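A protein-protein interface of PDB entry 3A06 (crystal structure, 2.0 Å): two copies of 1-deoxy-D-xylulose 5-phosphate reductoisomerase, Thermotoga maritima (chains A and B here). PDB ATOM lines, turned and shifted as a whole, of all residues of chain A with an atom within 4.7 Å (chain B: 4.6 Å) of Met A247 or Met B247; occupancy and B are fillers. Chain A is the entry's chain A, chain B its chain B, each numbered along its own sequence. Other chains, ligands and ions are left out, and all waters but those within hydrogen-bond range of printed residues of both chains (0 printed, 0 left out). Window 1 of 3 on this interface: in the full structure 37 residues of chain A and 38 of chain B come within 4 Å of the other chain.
Met A247 touches just these residues of chain B: Val B245 (3.7 Å), Lys B246 (3.4 Å) and Met B247 (2.8 Å). Met B247 touches just these residues of chain A: Val A245, Lys A246, Met A247 and Leu A275. Of the printed residues of chain A, Lys B246 touches Met A247. Printed residues of chain B within 4 Å of Val A245: Met B247, Val B248 and Val B249. Ala A237 touches none of the printed residues of chain B. Ala B237 touches none of the printed residues of chain A. The nearest residue of chain B that does not touch Met A247 is Val B249 (4.2 Å).
Of the 10 printed residues of chain A, 6 touch a printed residue of chain B. Hydrophobic or aromatic side chains of chain A that line the printed part of chain B: Val A245, Met A247, Val A248 and Leu A275. Of the 9 printed residues of chain B, 6 touch a printed residue of chain A. Among the printed residues, 12 pairs touch across the chains. Among the printed residues, no Asp or Glu carboxylate lies within 4 Å of a Lys or Arg side-chain nitrogen of the other chain.
Val A245 touches Met B247, and with the chains exchanged Met A247 touches Val B245. Val A245 touches Val B249, and with the chains exchanged Val A249 touches Val B245. Lys A246 touches Met B247, and with the chains exchanged Met A247 touches Lys B246. Met A247 touches its own counterpart, Met B247. Of the 12 pairs that touch across the chains among the printed residues, 9 have their exchanged pair printed and touching as well.
Among the printed residues, pairs that only touch across the chains: Val A245 with Val B248 (3.3 Å), Val A248 with Val B245 (3.3 Å), Lys A246 with Met B247 (3.3 Å), Met A247 with Lys B246 (3.4 Å), Val A245 with Met B247 (3.5 Å), Met A247 with Val B245 (3.7 Å), Leu A275 with Val B245 (3.8 Å), Leu A275 with Met B247 (3.8 Å) and Leu A275 with Phe B282 (3.99 Å).
O of Gly A236 is in hydrogen-bond range of N of Val A248 (3.0 Å). N of Val B248 is in hydrogen-bond range of O of Gly B236, at 3.0 Å.
O of Val A249 is in hydrogen-bond range of N of Val B245, at 2.7 Å. N of Val A245 sits at hydrogen-bond distance from O of Val B249 (2.7 Å). The backbone NH of Met A247 lies within hydrogen-bond range of the backbone carbonyl oxygen of Met B247 (2.8 Å).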
ATOM      1  N   VAL A 234      -5.144  28.014  17.842  1.00  0.00           N
ATOM      2  CA  VAL A 234      -5.080  26.724  17.133  1.00  0.00           C
ATOM      3  C   VAL A 234      -4.942  25.601  18.156  1.00  0.00           C
ATOM      4  O   VAL A 234      -3.951  25.572  18.914  1.00  0.00           O
ATOM      5  CB  VAL A 234      -3.880  26.679  16.179  1.00  0.00           C
ATOM      6  CG1 VAL A 234      -3.753  25.296  15.508  1.00  0.00           C
ATOM      7  CG2 VAL A 234      -4.002  27.766  15.111  1.00  0.00           C
ATOM      8  N   GLY A 236      -5.322  22.162  17.258  1.00  0.00           N
ATOM      9  CA  GLY A 236      -4.766  20.977  16.637  1.00  0.00           C
ATOM     10  C   GLY A 236      -4.755  21.194  15.150  1.00  0.00           C
ATOM     11  O   GLY A 236      -5.548  22.002  14.628  1.00  0.00           O
ATOM     12  N   ALA A 237      -3.846  20.505  14.465  1.00  0.00           N
ATOM     13  CA  ALA A 237      -3.771  20.587  13.014  1.00  0.00           C
ATOM     14  C   ALA A 237      -3.350  19.229  12.494  1.00  0.00           C
ATOM     15  O   ALA A 237      -2.636  18.479  13.187  1.00  0.00           O
ATOM     16  CB  ALA A 237      -2.768  21.680  12.590  1.00  0.00           C
ATOM     17  N   VAL A 245      -3.439  21.519   4.901  1.00  0.00           N
ATOM     18  CA  VAL A 245      -3.424  21.433   6.363  1.00  0.00           C
ATOM     19  C   VAL A 245      -4.814  21.777   6.870  1.00  0.00           C
ATOM     20  O   VAL A 245      -5.354  22.826   6.509  1.00  0.00           O
ATOM     21  CB  VAL A 245      -2.385  22.424   6.999  1.00  0.00           C
ATOM     22  CG1 VAL A 245      -2.321  22.252   8.516  1.00  0.00           C
ATOM     23  CG2 VAL A 245      -1.035  22.153   6.445  1.00  0.00           C
ATOM     24  N   LYS A 246      -5.422  20.869   7.646  1.00  0.00           N
ATOM     25  CA  LYS A 246      -6.696  21.156   8.318  1.00  0.00           C
ATOM     26  C   LYS A 246      -6.382  21.565   9.750  1.00  0.00           C
ATOM     27  O   LYS A 246      -5.693  20.819  10.491  1.00  0.00           O
ATOM     28  CB  LYS A 246      -7.639  19.932   8.279  1.00  0.00           C
ATOM     29  CG  LYS A 246      -7.977  19.458   6.851  1.00  0.00           C
ATOM     30  CD  LYS A 246      -9.159  18.475   6.784  1.00  0.00           C
ATOM     31  CE  LYS A 246      -8.759  17.084   7.085  1.00  0.00           C
ATOM     32  NZ  LYS A 246     -10.007  16.215   7.336  1.00  0.00           N
ATOM     33  N   MET A 247      -6.852  22.744  10.134  1.00  0.00           N
ATOM     34  CA  MET A 247      -6.587  23.276  11.464  1.00  0.00           C
ATOM     35  C   MET A 247      -7.916  23.547  12.133  1.00  0.00           C
ATOM     36  O   MET A 247      -8.896  23.876  11.452  1.00  0.00           O
ATOM     37  CB  MET A 247      -5.843  24.613  11.420  1.00  0.00           C
ATOM     38  CG  MET A 247      -4.691  24.762  10.437  1.00  0.00           C
ATOM     39  SD  MET A 247      -3.747  26.202  10.984  1.00  0.00           S
ATOM     40  CE  MET A 247      -4.929  27.554  10.801  1.00  0.00           C
ATOM     41  N   VAL A 248      -7.936  23.439  13.457  1.00  0.00           N
ATOM     42  CA  VAL A 248      -9.116  23.783  14.240  1.00  0.00           C
ATOM     43  C   VAL A 248      -8.766  24.957  15.159  1.00  0.00           C
ATOM     44  O   VAL A 248      -7.760  24.904  15.897  1.00  0.00           O
ATOM     45  CB  VAL A 248      -9.668  22.594  15.049  1.00  0.00           C
ATOM     46  CG1 VAL A 248     -10.838  23.041  15.909  1.00  0.00           C
ATOM     47  CG2 VAL A 248     -10.155  21.471  14.094  1.00  0.00           C
ATOM     48  N   VAL A 249      -9.578  26.016  15.086  1.00  0.00           N
ATOM     49  CA  VAL A 249      -9.394  27.190  15.920  1.00  0.00           C
ATOM     50  C   VAL A 249     -10.615  27.352  16.811  1.00  0.00           C
ATOM     51  O   VAL A 249     -11.724  27.058  16.380  1.00  0.00           O
ATOM     52  CB  VAL A 249      -9.246  28.438  15.030  1.00  0.00           C
ATOM     53  CG1 VAL A 249      -9.301  29.706  15.847  1.00  0.00           C
ATOM     54  CG2 VAL A 249      -7.949  28.362  14.246  1.00  0.00           C
ATOM     55  N   LEU A 275     -14.124  35.225  12.456  1.00  0.00           N
ATOM     56  CA  LEU A 275     -12.824  35.424  11.813  1.00  0.00           C
ATOM     57  C   LEU A 275     -12.373  36.878  11.834  1.00  0.00           C
ATOM     58  O   LEU A 275     -13.127  37.772  11.455  1.00  0.00           O
ATOM     59  CB  LEU A 275     -12.873  34.920  10.360  1.00  0.00           C
ATOM     60  CG  LEU A 275     -12.210  33.567  10.069  1.00  0.00           C
ATOM     61  CD1 LEU A 275     -12.677  32.477  11.019  1.00  0.00           C
ATOM     62  CD2 LEU A 275     -12.438  33.147   8.634  1.00  0.00           C
ATOM     63  N   LEU A 280      -0.488  33.904  14.531  1.00  0.00           N
ATOM     64  CA  LEU A 280      -0.304  32.492  14.805  1.00  0.00           C
ATOM     65  C   LEU A 280       1.170  32.138  14.802  1.00  0.00           C
ATOM     66  O   LEU A 280       1.786  32.014  13.748  1.00  0.00           O
ATOM     67  CB  LEU A 280      -1.089  31.626  13.808  1.00  0.00           C
ATOM     68  CG  LEU A 280      -2.619  31.777  13.746  1.00  0.00           C
ATOM     69  CD1 LEU A 280      -3.209  30.788  12.769  1.00  0.00           C
ATOM     70  CD2 LEU A 280      -3.287  31.617  15.111  1.00  0.00           C
ATOM     71  N   VAL B 234      -5.133  30.557   3.705  1.00  0.00           N
ATOM     72  CA  VAL B 234      -6.417  29.920   4.012  1.00  0.00           C
ATOM     73  C   VAL B 234      -7.272  29.943   2.734  1.00  0.00           C
ATOM     74  O   VAL B 234      -7.492  31.014   2.153  1.00  0.00           O
ATOM     75  CB  VAL B 234      -7.118  30.626   5.186  1.00  0.00           C
ATOM     76  CG1 VAL B 234      -8.570  30.126   5.373  1.00  0.00           C
ATOM     77  CG2 VAL B 234      -6.305  30.444   6.475  1.00  0.00           C
ATOM     78  N   GLY B 236     -10.295  28.246   2.650  1.00  0.00           N
ATOM     79  CA  GLY B 236     -11.670  28.139   3.070  1.00  0.00           C
ATOM     80  C   GLY B 236     -11.752  27.778   4.540  1.00  0.00           C
ATOM     81  O   GLY B 236     -10.807  27.201   5.077  1.00  0.00           O
ATOM     82  N   ALA B 237     -12.885  28.105   5.153  1.00  0.00           N
ATOM     83  CA  ALA B 237     -13.145  27.834   6.565  1.00  0.00           C
ATOM     84  C   ALA B 237     -14.632  27.592   6.784  1.00  0.00           C
ATOM     85  O   ALA B 237     -15.472  28.098   6.019  1.00  0.00           O
ATOM     86  CB  ALA B 237     -12.660  29.017   7.421  1.00  0.00           C
ATOM     87  N   VAL B 245     -13.776  26.592  14.659  1.00  0.00           N
ATOM     88  CA  VAL B 245     -13.656  26.975  13.250  1.00  0.00           C
ATOM     89  C   VAL B 245     -12.716  25.949  12.637  1.00  0.00           C
ATOM     90  O   VAL B 245     -11.648  25.674  13.208  1.00  0.00           O
ATOM     91  CB  VAL B 245     -13.035  28.393  13.074  1.00  0.00           C
ATOM     92  CG1 VAL B 245     -12.867  28.744  11.558  1.00  0.00           C
ATOM     93  CG2 VAL B 245     -13.914  29.462  13.749  1.00  0.00           C
ATOM     94  N   LYS B 246     -13.122  25.324  11.535  1.00  0.00           N
ATOM     95  CA  LYS B 246     -12.222  24.418  10.809  1.00  0.00           C
ATOM     96  C   LYS B 246     -11.727  25.152   9.574  1.00  0.00           C
ATOM     97  O   LYS B 246     -12.543  25.633   8.782  1.00  0.00           O
ATOM     98  CB  LYS B 246     -12.925  23.131  10.383  1.00  0.00           C
ATOM     99  CG  LYS B 246     -13.546  22.333  11.555  1.00  0.00           C
ATOM    100  CD  LYS B 246     -13.941  20.903  11.116  1.00  0.00           C
ATOM    101  CE  LYS B 246     -15.391  20.841  10.692  1.00  0.00           C
ATOM    102  NZ  LYS B 246     -15.770  19.533  10.013  1.00  0.00           N
ATOM    103  N   MET B 247     -10.410  25.234   9.431  1.00  0.00           N
ATOM    104  CA  MET B 247      -9.760  25.958   8.329  1.00  0.00           C
ATOM    105  C   MET B 247      -8.867  25.039   7.528  1.00  0.00           C
ATOM    106  O   MET B 247      -8.253  24.108   8.090  1.00  0.00           O
ATOM    107  CB  MET B 247      -8.848  27.053   8.868  1.00  0.00           C
ATOM    108  CG  MET B 247      -9.506  28.203   9.521  1.00  0.00           C
ATOM    109  SD  MET B 247      -8.253  29.475   9.899  1.00  0.00           S
ATOM    110  CE  MET B 247      -9.305  30.790  10.471  1.00  0.00           C
ATOM    111  N   VAL B 248      -8.771  25.312   6.227  1.00  0.00           N
ATOM    112  CA  VAL B 248      -7.914  24.552   5.332  1.00  0.00           C
ATOM    113  C   VAL B 248      -6.856  25.495   4.778  1.00  0.00           C
ATOM    114  O   VAL B 248      -7.178  26.512   4.186  1.00  0.00           O
ATOM    115  CB  VAL B 248      -8.717  23.878   4.207  1.00  0.00           C
ATOM    116  CG1 VAL B 248      -7.788  23.121   3.257  1.00  0.00           C
ATOM    117  CG2 VAL B 248      -9.791  22.914   4.806  1.00  0.00           C
ATOM    118  N   VAL B 249      -5.595  25.162   5.015  1.00  0.00           N
ATOM    119  CA  VAL B 249      -4.454  25.967   4.582  1.00  0.00           C
ATOM    120  C   VAL B 249      -3.660  25.155   3.576  1.00  0.00           C
ATOM    121  O   VAL B 249      -3.518  23.933   3.736  1.00  0.00           O
ATOM    122  CB  VAL B 249      -3.551  26.304   5.791  1.00  0.00           C
ATOM    123  CG1 VAL B 249      -2.186  26.790   5.348  1.00  0.00           C
ATOM    124  CG2 VAL B 249      -4.214  27.333   6.680  1.00  0.00           C
ATOM    125  N   PHE B 282      -8.175  38.879   7.672  1.00  0.00           N
ATOM    126  CA  PHE B 282      -9.529  38.694   7.143  1.00  0.00           C
ATOM    127  C   PHE B 282     -10.272  40.030   7.225  1.00  0.00           C
ATOM    128  O   PHE B 282     -10.537  40.540   8.326  1.00  0.00           O
ATOM    129  CB  PHE B 282     -10.279  37.598   7.918  1.00  0.00           C
ATOM    130  CG  PHE B 282      -9.572  36.275   7.926  1.00  0.00           C
ATOM    131  CD1 PHE B 282      -8.788  35.902   9.011  1.00  0.00           C
ATOM    132  CD2 PHE B 282      -9.678  35.406   6.843  1.00  0.00           C
ATOM    133  CE1 PHE B 282      -8.117  34.682   9.038  1.00  0.00           C
ATOM    134  CE2 PHE B 282      -9.009  34.181   6.844  1.00  0.00           C
ATOM    135  CZ  PHE B 282      -8.217  33.816   7.963  1.00  0.00           C
